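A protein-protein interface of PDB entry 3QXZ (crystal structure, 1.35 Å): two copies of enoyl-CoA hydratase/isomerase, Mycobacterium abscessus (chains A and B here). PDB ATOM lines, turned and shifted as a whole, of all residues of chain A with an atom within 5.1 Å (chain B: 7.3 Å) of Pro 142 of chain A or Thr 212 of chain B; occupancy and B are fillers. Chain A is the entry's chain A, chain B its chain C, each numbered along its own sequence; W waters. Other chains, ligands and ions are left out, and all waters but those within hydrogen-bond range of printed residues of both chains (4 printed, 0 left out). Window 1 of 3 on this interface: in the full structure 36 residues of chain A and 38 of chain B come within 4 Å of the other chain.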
ATOM      1  N   ILE A 133       9.394 -28.182  16.613  1.00  0.00           N
ATOM      2  CA  ILE A 133       8.157 -28.268  15.818  1.00  0.00           C
ATOM      3  C   ILE A 133       8.225 -27.060  14.875  1.00  0.00           C
ATOM      4  O   ILE A 133       7.606 -26.035  15.135  1.00  0.00           O
ATOM      5  CB  ILE A 133       6.905 -28.257  16.726  1.00  0.00           C
ATOM      6  CG1 ILE A 133       6.987 -29.392  17.750  1.00  0.00           C
ATOM      7  CG2 ILE A 133       5.633 -28.385  15.911  1.00  0.00           C
ATOM      8  CD1 ILE A 133       5.952 -29.261  18.899  1.00  0.00           C
ATOM      9  N   GLN A 135       7.359 -26.383  11.704  1.00  0.00           N
ATOM     10  CA  GLN A 135       6.504 -26.290  10.506  1.00  0.00           C
ATOM     11  C   GLN A 135       6.236 -24.849  10.048  1.00  0.00           C
ATOM     12  O   GLN A 135       6.215 -24.577   8.842  1.00  0.00           O
ATOM     13  CB  GLN A 135       5.174 -26.986  10.794  1.00  0.00           C
ATOM     14  CG  GLN A 135       5.193 -28.531  10.685  1.00  0.00           C
ATOM     15  CD  GLN A 135       5.581 -29.247  11.981  1.00  0.00           C
ATOM     16  OE1 GLN A 135       6.410 -28.769  12.762  1.00  0.00           O
ATOM     17  NE2 GLN A 135       4.968 -30.405  12.217  1.00  0.00           N
ATOM     18  N   VAL A 136       5.997 -23.924  10.983  1.00  0.00           N
ATOM     19  CA  VAL A 136       5.686 -22.532  10.562  1.00  0.00           C
ATOM     20  C   VAL A 136       6.853 -21.844   9.855  1.00  0.00           C
ATOM     21  O   VAL A 136       6.629 -20.916   9.076  1.00  0.00           O
ATOM     22  CB  VAL A 136       5.196 -21.623  11.729  1.00  0.00           C
ATOM     23  CG1 VAL A 136       3.881 -22.152  12.335  1.00  0.00           C
ATOM     24  CG2 VAL A 136       6.300 -21.444  12.797  1.00  0.00           C
ATOM     25  N   VAL A 140       4.062 -24.059   6.427  1.00  0.00           N
ATOM     26  CA  VAL A 140       2.901 -24.862   6.844  1.00  0.00           C
ATOM     27  C   VAL A 140       2.618 -24.610   8.339  1.00  0.00           C
ATOM     28  O   VAL A 140       2.784 -23.498   8.780  1.00  0.00           O
ATOM     29  CB  VAL A 140       2.993 -26.334   6.404  1.00  0.00           C
ATOM     30  CG1 VAL A 140       2.781 -26.418   4.864  1.00  0.00           C
ATOM     31  CG2 VAL A 140       4.291 -26.986   6.813  1.00  0.00           C
ATOM     32  N   ALA A 141       2.140 -25.592   9.105  1.00  0.00           N
ATOM     33  CA  ALA A 141       1.730 -25.323  10.484  1.00  0.00           C
ATOM     34  C   ALA A 141       1.841 -26.607  11.254  1.00  0.00           C
ATOM     35  O   ALA A 141       1.993 -27.672  10.667  1.00  0.00           O
ATOM     36  CB  ALA A 141       0.311 -24.782  10.524  1.00  0.00           C
ATOM     37  N   PRO A 142       1.774 -26.535  12.596  1.00  0.00           N
ATOM     38  CA  PRO A 142       1.861 -27.774  13.383  1.00  0.00           C
ATOM     39  C   PRO A 142       0.730 -28.729  13.010  1.00  0.00           C
ATOM     40  O   PRO A 142      -0.353 -28.307  12.584  1.00  0.00           O
ATOM     41  CB  PRO A 142       1.732 -27.279  14.843  1.00  0.00           C
ATOM     42  CG  PRO A 142       2.211 -25.822  14.786  1.00  0.00           C
ATOM     43  CD  PRO A 142       1.689 -25.330  13.447  1.00  0.00           C
ATOM     44  N   ASP A 143       1.013 -30.012  13.158  1.00  0.00           N
ATOM     45  CA  ASP A 143       0.147 -31.081  12.691  1.00  0.00           C
ATOM     46  C   ASP A 143      -0.059 -32.116  13.800  1.00  0.00           C
ATOM     47  O   ASP A 143       0.439 -31.979  14.928  1.00  0.00           O
ATOM     48  CB  ASP A 143       0.747 -31.688  11.392  1.00  0.00           C
ATOM     49  CG  ASP A 143       2.225 -31.998  11.536  1.00  0.00           C
ATOM     50  OD1 ASP A 143       2.675 -32.322  12.643  1.00  0.00           O
ATOM     51  OD2 ASP A 143       2.957 -31.900  10.523  1.00  0.00           O
ATOM     52  N   ALA A 144      -0.814 -33.149  13.442  1.00  0.00           N
ATOM     53  CA  ALA A 144      -1.096 -34.292  14.321  1.00  0.00           C
ATOM     54  C   ALA A 144      -1.544 -33.836  15.713  1.00  0.00           C
ATOM     55  O   ALA A 144      -1.086 -34.357  16.737  1.00  0.00           O
ATOM     56  CB  ALA A 144       0.119 -35.198  14.419  1.00  0.00           C
ATOM     57  N   ALA A 146      -0.988 -31.207  17.463  1.00  0.00           N
ATOM     58  CA  ALA A 146      -0.103 -30.470  18.366  1.00  0.00           C
ATOM     59  C   ALA A 146      -0.761 -29.251  18.987  1.00  0.00           C
ATOM     60  O   ALA A 146      -0.411 -28.856  20.110  1.00  0.00           O
ATOM     61  CB  ALA A 146       1.141 -30.039  17.633  1.00  0.00           C
ATOM     62  N   HIS A 147      -1.705 -28.607  18.296  1.00  0.00           N
ATOM     63  CA  HIS A 147      -2.387 -27.430  18.873  1.00  0.00           C
ATOM     64  C   HIS A 147      -3.188 -27.781  20.135  1.00  0.00           C
ATOM     65  O   HIS A 147      -3.518 -26.881  20.907  1.00  0.00           O
ATOM     66  CB  HIS A 147      -3.342 -26.762  17.861  1.00  0.00           C
ATOM     67  CG  HIS A 147      -2.673 -26.195  16.635  1.00  0.00           C
ATOM     68  ND1 HIS A 147      -2.367 -26.963  15.529  1.00  0.00           N
ATOM     69  CD2 HIS A 147      -2.301 -24.925  16.328  1.00  0.00           C
ATOM     70  CE1 HIS A 147      -1.814 -26.188  14.596  1.00  0.00           C
ATOM     71  NE2 HIS A 147      -1.756 -24.946  15.055  1.00  0.00           N
ATOM     72  N   LEU A 163       5.336 -23.428  19.019  1.00  0.00           N
ATOM     73  CA  LEU A 163       4.558 -23.521  17.756  1.00  0.00           C
ATOM     74  C   LEU A 163       4.704 -22.302  16.858  1.00  0.00           C
ATOM     75  O   LEU A 163       4.733 -22.444  15.625  1.00  0.00           O
ATOM     76  CB  LEU A 163       3.082 -23.762  18.053  1.00  0.00           C
ATOM     77  CG  LEU A 163       2.784 -25.039  18.856  1.00  0.00           C
ATOM     78  CD1 LEU A 163       1.269 -25.182  18.991  1.00  0.00           C
ATOM     79  CD2 LEU A 163       3.416 -26.271  18.209  1.00  0.00           C
ATOM     80  N   LEU A 164       4.789 -21.107  17.439  1.00  0.00           N
ATOM     81  CA  LEU A 164       4.838 -19.876  16.650  1.00  0.00           C
ATOM     82  C   LEU A 164       6.248 -19.538  16.213  1.00  0.00           C
ATOM     83  O   LEU A 164       6.417 -18.865  15.187  1.00  0.00           O
ATOM     84  CB  LEU A 164       4.233 -18.697  17.421  1.00  0.00           C
ATOM     85  CG  LEU A 164       2.751 -18.771  17.773  1.00  0.00           C
ATOM     86  CD1 LEU A 164       2.305 -17.584  18.576  1.00  0.00           C
ATOM     87  CD2 LEU A 164       1.901 -18.867  16.487  1.00  0.00           C
ATOM     88  N   ARG B  98      -4.485 -12.155  15.054  1.00  0.00           N
ATOM     89  CA  ARG B  98      -3.760 -13.056  14.159  1.00  0.00           C
ATOM     90  C   ARG B  98      -2.263 -12.887  14.363  1.00  0.00           C
ATOM     91  O   ARG B  98      -1.495 -13.835  14.171  1.00  0.00           O
ATOM     92  CB  ARG B  98      -4.137 -12.787  12.703  1.00  0.00           C
ATOM     93  CG  ARG B  98      -5.583 -13.183  12.387  1.00  0.00           C
ATOM     94  CD  ARG B  98      -6.072 -12.586  11.036  1.00  0.00           C
ATOM     95  NE  ARG B  98      -5.747 -11.157  10.848  1.00  0.00           N
ATOM     96  CZ  ARG B  98      -6.520 -10.122  11.195  1.00  0.00           C
ATOM     97  NH1 ARG B  98      -7.715 -10.300  11.753  1.00  0.00           N
ATOM     98  NH2 ARG B  98      -6.094  -8.884  10.978  1.00  0.00           N
ATOM     99  N   PRO B 206       4.019 -15.541   7.375  1.00  0.00           N
ATOM    100  CA  PRO B 206       2.930 -14.776   7.996  1.00  0.00           C
ATOM    101  C   PRO B 206       1.650 -15.568   8.243  1.00  0.00           C
ATOM    102  O   PRO B 206       1.077 -15.497   9.343  1.00  0.00           O
ATOM    103  CB  PRO B 206       2.690 -13.613   7.016  1.00  0.00           C
ATOM    104  CG  PRO B 206       4.041 -13.413   6.384  1.00  0.00           C
ATOM    105  CD  PRO B 206       4.649 -14.789   6.268  1.00  0.00           C
ATOM    106  N   GLU B 207       1.158 -16.299   7.247  1.00  0.00           N
ATOM    107  CA  GLU B 207      -0.106 -16.986   7.432  1.00  0.00           C
ATOM    108  C   GLU B 207       0.048 -18.226   8.310  1.00  0.00           C
ATOM    109  O   GLU B 207      -0.888 -18.620   9.003  1.00  0.00           O
ATOM    110  CB  GLU B 207      -0.724 -17.358   6.081  1.00  0.00           C
ATOM    111  CG  GLU B 207      -2.219 -17.737   6.142  1.00  0.00           C
ATOM    112  CD  GLU B 207      -3.136 -16.573   6.556  1.00  0.00           C
ATOM    113  OE1 GLU B 207      -2.687 -15.393   6.643  1.00  0.00           O
ATOM    114  OE2 GLU B 207      -4.336 -16.850   6.779  1.00  0.00           O
ATOM    115  N   SER B 208       1.225 -18.844   8.280  1.00  0.00           N
ATOM    116  CA  SER B 208       1.553 -19.920   9.210  1.00  0.00           C
ATOM    117  C   SER B 208       1.416 -19.453  10.652  1.00  0.00           C
ATOM    118  O   SER B 208       0.752 -20.118  11.457  1.00  0.00           O
ATOM    119  CB  SER B 208       2.975 -20.394   8.969  1.00  0.00           C
ATOM    120  OG  SER B 208       3.061 -21.011   7.698  1.00  0.00           O
ATOM    121  N   ALA B 209       2.018 -18.320  10.999  1.00  0.00           N
ATOM    122  CA  ALA B 209       1.887 -17.805  12.369  1.00  0.00           C
ATOM    123  C   ALA B 209       0.424 -17.464  12.688  1.00  0.00           C
ATOM    124  O   ALA B 209      -0.045 -17.765  13.807  1.00  0.00           O
ATOM    125  CB  ALA B 209       2.777 -16.586  12.553  1.00  0.00           C
ATOM    126  N   ALA B 210      -0.299 -16.837  11.749  1.00  0.00           N
ATOM    127  CA  ALA B 210      -1.664 -16.421  12.033  1.00  0.00           C
ATOM    128  C   ALA B 210      -2.580 -17.603  12.316  1.00  0.00           C
ATOM    129  O   ALA B 210      -3.342 -17.601  13.296  1.00  0.00           O
ATOM    130  CB  ALA B 210      -2.224 -15.581  10.878  1.00  0.00           C
ATOM    131  N   LEU B 211      -2.544 -18.613  11.455  1.00  0.00           N
ATOM    132  CA  LEU B 211      -3.440 -19.748  11.638  1.00  0.00           C
ATOM    133  C   LEU B 211      -3.093 -20.563  12.876  1.00  0.00           C
ATOM    134  O   LEU B 211      -3.996 -21.051  13.589  1.00  0.00           O
ATOM    135  CB  LEU B 211      -3.450 -20.617  10.388  1.00  0.00           C
ATOM    136  CG  LEU B 211      -4.022 -19.956   9.132  1.00  0.00           C
ATOM    137  CD1 LEU B 211      -3.947 -20.922   7.951  1.00  0.00           C
ATOM    138  CD2 LEU B 211      -5.463 -19.475   9.352  1.00  0.00           C
ATOM    139  N   THR B 212      -1.791 -20.707  13.142  1.00  0.00           N
ATOM    140  CA  THR B 212      -1.335 -21.440  14.317  1.00  0.00           C
ATOM    141  C   THR B 212      -1.776 -20.717  15.591  1.00  0.00           C
ATOM    142  O   THR B 212      -2.338 -21.339  16.501  1.00  0.00           O
ATOM    143  CB  THR B 212       0.189 -21.592  14.268  1.00  0.00           C
ATOM    144  OG1 THR B 212       0.547 -22.363  13.098  1.00  0.00           O
ATOM    145  CG2 THR B 212       0.705 -22.311  15.500  1.00  0.00           C
ATOM    146  N   LYS B 213      -1.547 -19.404  15.642  1.00  0.00           N
ATOM    147  CA  LYS B 213      -1.964 -18.640  16.806  1.00  0.00           C
ATOM    148  C   LYS B 213      -3.474 -18.759  17.026  1.00  0.00           C
ATOM    149  O   LYS B 213      -3.945 -18.983  18.157  1.00  0.00           O
ATOM    150  CB  LYS B 213      -1.544 -17.167  16.693  1.00  0.00           C
ATOM    151  CG  LYS B 213      -2.059 -16.347  17.881  1.00  0.00           C
ATOM    152  CD  LYS B 213      -1.517 -14.936  17.928  1.00  0.00           C
ATOM    153  CE  LYS B 213      -2.190 -14.195  19.092  1.00  0.00           C
ATOM    154  NZ  LYS B 213      -1.398 -12.977  19.515  1.00  0.00           N
ATOM    155  N   ARG B 214      -4.247 -18.577  15.961  1.00  0.00           N
ATOM    156  CA  ARG B 214      -5.699 -18.556  16.092  1.00  0.00           C
ATOM    157  C   ARG B 214      -6.259 -19.921  16.488  1.00  0.00           C
ATOM    158  O   ARG B 214      -7.217 -19.976  17.254  1.00  0.00           O
ATOM    159  CB  ARG B 214      -6.383 -17.984  14.843  1.00  0.00           C
ATOM    160  CG  ARG B 214      -6.174 -16.491  14.737  1.00  0.00           C
ATOM    161  CD  ARG B 214      -7.317 -15.652  15.348  1.00  0.00           C
ATOM    162  NE  ARG B 214      -7.898 -16.153  16.602  1.00  0.00           N
ATOM    163  CZ  ARG B 214      -7.361 -15.998  17.811  1.00  0.00           C
ATOM    164  NH1 ARG B 214      -6.185 -15.389  17.980  1.00  0.00           N
ATOM    165  NH2 ARG B 214      -8.006 -16.486  18.867  1.00  0.00           N
ATOM    166  N   LEU B 215      -5.661 -21.018  16.024  1.00  0.00           N
ATOM    167  CA  LEU B 215      -6.156 -22.328  16.414  1.00  0.00           C
ATOM    168  C   LEU B 215      -5.779 -22.626  17.865  1.00  0.00           C
ATOM    169  O   LEU B 215      -6.622 -23.104  18.651  1.00  0.00           O
ATOM    170  CB  LEU B 215      -5.656 -23.416  15.463  1.00  0.00           C
ATOM    171  CG  LEU B 215      -6.190 -24.821  15.784  1.00  0.00           C
ATOM    172  CD1 LEU B 215      -7.732 -24.864  15.986  1.00  0.00           C
ATOM    173  CD2 LEU B 215      -5.778 -25.790  14.680  1.00  0.00           C
ATOM    174  N   LEU B 216      -4.541 -22.322  18.232  1.00  0.00           N
ATOM    175  CA  LEU B 216      -4.107 -22.548  19.607  1.00  0.00           C
ATOM    176  C   LEU B 216      -5.080 -21.848  20.562  1.00  0.00           C
ATOM    177  O   LEU B 216      -5.588 -22.481  21.527  1.00  0.00           O
ATOM    178  CB  LEU B 216      -2.671 -22.030  19.788  1.00  0.00           C
ATOM    179  CG  LEU B 216      -2.144 -22.111  21.221  1.00  0.00           C
ATOM    180  CD1 LEU B 216      -1.858 -23.531  21.665  1.00  0.00           C
ATOM    181  CD2 LEU B 216      -0.868 -21.306  21.292  1.00  0.00           C
ATOM    182  N   TRP B 217      -5.319 -20.557  20.335  1.00  0.00           N
ATOM    183  CA  TRP B 217      -6.152 -19.807  21.262  1.00  0.00           C
ATOM    184  C   TRP B 217      -7.643 -20.051  21.078  1.00  0.00           C
ATOM    185  O   TRP B 217      -8.351 -20.146  22.089  1.00  0.00           O
ATOM    186  CB  TRP B 217      -5.827 -18.316  21.153  1.00  0.00           C
ATOM    187  CG  TRP B 217      -4.541 -17.954  21.824  1.00  0.00           C
ATOM    188  CD1 TRP B 217      -3.374 -17.598  21.211  1.00  0.00           C
ATOM    189  CD2 TRP B 217      -4.308 -17.872  23.223  1.00  0.00           C
ATOM    190  NE1 TRP B 217      -2.418 -17.303  22.152  1.00  0.00           N
ATOM    191  CE2 TRP B 217      -2.973 -17.449  23.398  1.00  0.00           C
ATOM    192  CE3 TRP B 217      -5.112 -18.106  24.353  1.00  0.00           C
ATOM    193  CZ2 TRP B 217      -2.408 -17.263  24.667  1.00  0.00           C
ATOM    194  CZ3 TRP B 217      -4.555 -17.923  25.616  1.00  0.00           C
ATOM    195  CH2 TRP B 217      -3.215 -17.511  25.761  1.00  0.00           C
ATOM    196  N   ASP B 218      -8.145 -20.154  19.845  1.00  0.00           N
ATOM    197  CA  ASP B 218      -9.591 -20.420  19.709  1.00  0.00           C
ATOM    198  C   ASP B 218      -9.967 -21.726  20.423  1.00  0.00           C
ATOM    199  O   ASP B 218     -11.025 -21.807  21.041  1.00  0.00           O
ATOM    200  CB  ASP B 218     -10.022 -20.596  18.256  1.00  0.00           C
ATOM    201  CG  ASP B 218     -10.119 -19.320  17.484  1.00  0.00           C
ATOM    202  OD1 ASP B 218     -10.048 -18.197  18.048  1.00  0.00           O
ATOM    203  OD2 ASP B 218     -10.263 -19.463  16.243  1.00  0.00           O
ATOM    204  N   ARG B 232      -9.738 -28.624  12.025  1.00  0.00           N
ATOM    205  CA  ARG B 232      -9.223 -27.311  11.637  1.00  0.00           C
ATOM    206  C   ARG B 232      -7.765 -27.367  11.207  1.00  0.00           C
ATOM    207  O   ARG B 232      -7.381 -26.660  10.254  1.00  0.00           O
ATOM    208  CB  ARG B 232      -9.459 -26.193  12.647  1.00  0.00           C
ATOM    209  CG  ARG B 232      -9.420 -24.838  11.849  1.00  0.00           C
ATOM    210  CD  ARG B 232      -9.116 -23.591  12.650  1.00  0.00           C
ATOM    211  NE  ARG B 232     -10.189 -23.292  13.578  1.00  0.00           N
ATOM    212  CZ  ARG B 232     -10.173 -22.227  14.377  1.00  0.00           C
ATOM    213  NH1 ARG B 232     -11.198 -22.034  15.191  1.00  0.00           N
ATOM    214  NH2 ARG B 232      -9.127 -21.398  14.390  1.00  0.00           N
ATOM    215  N   GLU B 233      -6.942 -28.187  11.852  1.00  0.00           N
ATOM    216  CA  GLU B 233      -5.559 -28.347  11.363  1.00  0.00           C
ATOM    217  C   GLU B 233      -5.548 -28.773   9.898  1.00  0.00           C
ATOM    218  O   GLU B 233      -4.778 -28.257   9.080  1.00  0.00           O
ATOM    219  CB  GLU B 233      -4.804 -29.392  12.187  1.00  0.00           C
ATOM    220  CG  GLU B 233      -4.429 -28.945  13.565  1.00  0.00           C
ATOM    221  CD  GLU B 233      -3.661 -30.002  14.336  1.00  0.00           C
ATOM    222  OE1 GLU B 233      -3.664 -31.191  13.951  1.00  0.00           O
ATOM    223  OE2 GLU B 233      -3.053 -29.639  15.365  1.00  0.00           O
ATOM    224  N   THR B 234      -6.414 -29.717   9.537  1.00  0.00           N
ATOM    225  CA  THR B 234      -6.500 -30.140   8.153  1.00  0.00           C
ATOM    226  C   THR B 234      -6.954 -28.986   7.239  1.00  0.00           C
ATOM    227  O   THR B 234      -6.322 -28.748   6.197  1.00  0.00           O
ATOM    228  CB  THR B 234      -7.432 -31.342   8.034  1.00  0.00           C
ATOM    229  OG1 THR B 234      -6.805 -32.454   8.687  1.00  0.00           O
ATOM    230  CG2 THR B 234      -7.738 -31.687   6.544  1.00  0.00           C
ATOM    231  N   ASP B 236      -6.679 -25.724   7.779  1.00  0.00           N
ATOM    232  CA  ASP B 236      -5.599 -24.730   7.766  1.00  0.00           C
ATOM    233  C   ASP B 236      -4.451 -25.216   6.902  1.00  0.00           C
ATOM    234  O   ASP B 236      -3.884 -24.436   6.123  1.00  0.00           O
ATOM    235  CB  ASP B 236      -5.130 -24.443   9.198  1.00  0.00           C
ATOM    236  CG  ASP B 236      -6.109 -23.590   9.991  1.00  0.00           C
ATOM    237  OD1 ASP B 236      -7.082 -23.080   9.422  1.00  0.00           O
ATOM    238  OD2 ASP B 236      -5.865 -23.437  11.203  1.00  0.00           O
ATOM    239  N   HIS B 237      -4.124 -26.502   6.982  1.00  0.00           N
ATOM    240  CA  HIS B 237      -3.121 -27.057   6.073  1.00  0.00           C
ATOM    241  C   HIS B 237      -3.522 -26.915   4.616  1.00  0.00           C
ATOM    242  O   HIS B 237      -2.672 -26.521   3.805  1.00  0.00           O
ATOM    243  CB  HIS B 237      -2.807 -28.507   6.393  1.00  0.00           C
ATOM    244  CG  HIS B 237      -1.684 -28.661   7.358  1.00  0.00           C
ATOM    245  ND1 HIS B 237      -1.793 -28.347   8.693  1.00  0.00           N
ATOM    246  CD2 HIS B 237      -0.403 -29.065   7.169  1.00  0.00           C
ATOM    247  CE1 HIS B 237      -0.628 -28.549   9.287  1.00  0.00           C
ATOM    248  NE2 HIS B 237       0.230 -28.993   8.381  1.00  0.00           N
ATOM    249  N   LEU B 240      -2.787 -23.383   3.652  1.00  0.00           N
ATOM    250  CA  LEU B 240      -1.358 -23.068   3.556  1.00  0.00           C
ATOM    251  C   LEU B 240      -0.714 -23.777   2.383  1.00  0.00           C
ATOM    252  O   LEU B 240       0.146 -23.189   1.717  1.00  0.00           O
ATOM    253  CB  LEU B 240      -0.662 -23.400   4.878  1.00  0.00           C
ATOM    254  CG  LEU B 240      -1.176 -22.597   6.089  1.00  0.00           C
ATOM    255  CD1 LEU B 240      -0.683 -23.215   7.382  1.00  0.00           C
ATOM    256  CD2 LEU B 240      -0.700 -21.148   5.999  1.00  0.00           C
HETATM  257  O   HOH W   1      -2.535 -26.930  11.121  1.00  0.00           O
HETATM  258  O   HOH W   2       2.629 -30.265   8.355  1.00  0.00           O
HETATM  259  O   HOH W   3      -5.238 -25.146  22.272  1.00  0.00           O
HETATM  260  O   HOH W   4      -3.260 -24.367  12.053  1.00  0.00           O
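No position is printed for both chains.
Of the 20 pairs that touch across the chains among the printed residues, none has its exchanged pair printed and touching as well.
O of Val 140 of chain A lies within hydrogen-bond range of OG of Ser 208 of chain B, 2.7 Å away.
O of Ala 141 of chain A lies close to NE2 of His 237 of chain B (3.2 Å).
OE1 of Glu 233 of chain B is in hydrogen-bond range of N of Ala 144 of chain A (3.5 Å).
The backbone NH of Ala 146 of chain A sits at hydrogen-bond distance from the side-chain carboxylate of Glu 233 of chain B (3.3 Å).
The side-chain carboxylate of Glu 233 of chain B is in hydrogen-bond range of a ring nitrogen (ND1) of His 147 of chain A (2.8 Å).
Water W2 bridges NE2 of His 237 of chain B (2.7 Å) and OD2 of Asp 143 of chain A (2.7 Å).
Water W3 bridges O of Leu 216 of chain B and O of His 147 of chain A.
Water W4 lies within hydrogen-bond range of OD2 of Asp 236 of chain B (2.9 Å) and NE2 of His 147 of chain A (3.4 Å).
Water W1 lies within hydrogen-bond range of a ring nitrogen (ND1) of His 237 of chain B, the backbone carbonyl oxygen of Pro 142 of chain A and the backbone carbonyl oxygen of Glu 233 of chain B.
Ser 208 of chain B touches Val 136 of chain A (CB to O, 3.7 Å).
Val 136 of chain A touches Thr 212 of chain B.
Thr 212 of chain B touches Ala 141 of chain A.
Ala 141 of chain A touches Leu 240 of chain B.
CE1 of His 237 of chain B touches O of Pro 142 of chain A, 3.3 Å away.
Thr 212 of chain B touches His 147 of chain A (O to CD2, 3.6 Å).
Leu 215 of chain B touches His 147 of chain A.
His 147 of chain A touches Leu 216 of chain B (O to CD1, 3.8 Å).
CD2 of Leu 164 of chain A touches O of Ala 209 of chain B (3.5 Å).
Leu 164 of chain A touches Thr 212 of chain B (CD2 to CG2, 3.8 Å).
Printed residues of chain B that touch a printed residue of chain A: Ser 208, Ala 209, Thr 212, Lys 213, Leu 215, Leu 216, Glu 233, His 237 and Leu 240.
Of the 12 printed residues of chain A, 10 touch a printed residue of chain B.
Among the printed residues, 20 pairs touch across the chains.
The backbone carbonyl oxygen (O) of Gln 135 of chain A lies within hydrogen-bond range of the backbone NH (N) of Val 140 of chain A, at 3.3 Å.
The side-chain amide nitrogen of Gln 135 of chain A is in hydrogen-bond range of the side-chain carboxylate of Asp 143 of chain A (3.0 Å).
The backbone carbonyl oxygen of Ser 208 of chain B sits at hydrogen-bond distance from the side-chain hydroxyl of Thr 212 of chain B (2.8 Å).
O of Glu 233 of chain B is in hydrogen-bond range of ND1 of His 237 of chain B (3.0 Å).
Pro 142 of chain A touches two residues of chain B.
Thr 212 of chain B touches six residues of chain A.
Of the printed residues of chain A, Lys 213 of chain B touches Leu 164 (3.6 Å).
Of the printed residues of chain B, Val 140 of chain A touches Ser 208 (2.7 Å) and Leu 240 (3.7 Å).
Of the printed residues of chain A, Glu 233 of chain B touches Asp 143, Ala 144, Ala 146 and His 147.
Of the printed residues of chain A, Leu 215 of chain B touches His 147 (3.7 Å).
Of the printed residues of chain B, Ala 146 of chain A touches Glu 233 (3.3 Å).
Arg 232 of chain B touches none of the printed residues of chain A.
Ile 133 of chain A touches none of the printed residues of chain B.
The nearest residue of chain B that does not touch Pro 142 of chain A is Glu 233 of chain B (4.1 Å).
The nearest printed residue of chain A that does not touch Ser 208 of chain B is Ala 141 of chain A (4.8 Å).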
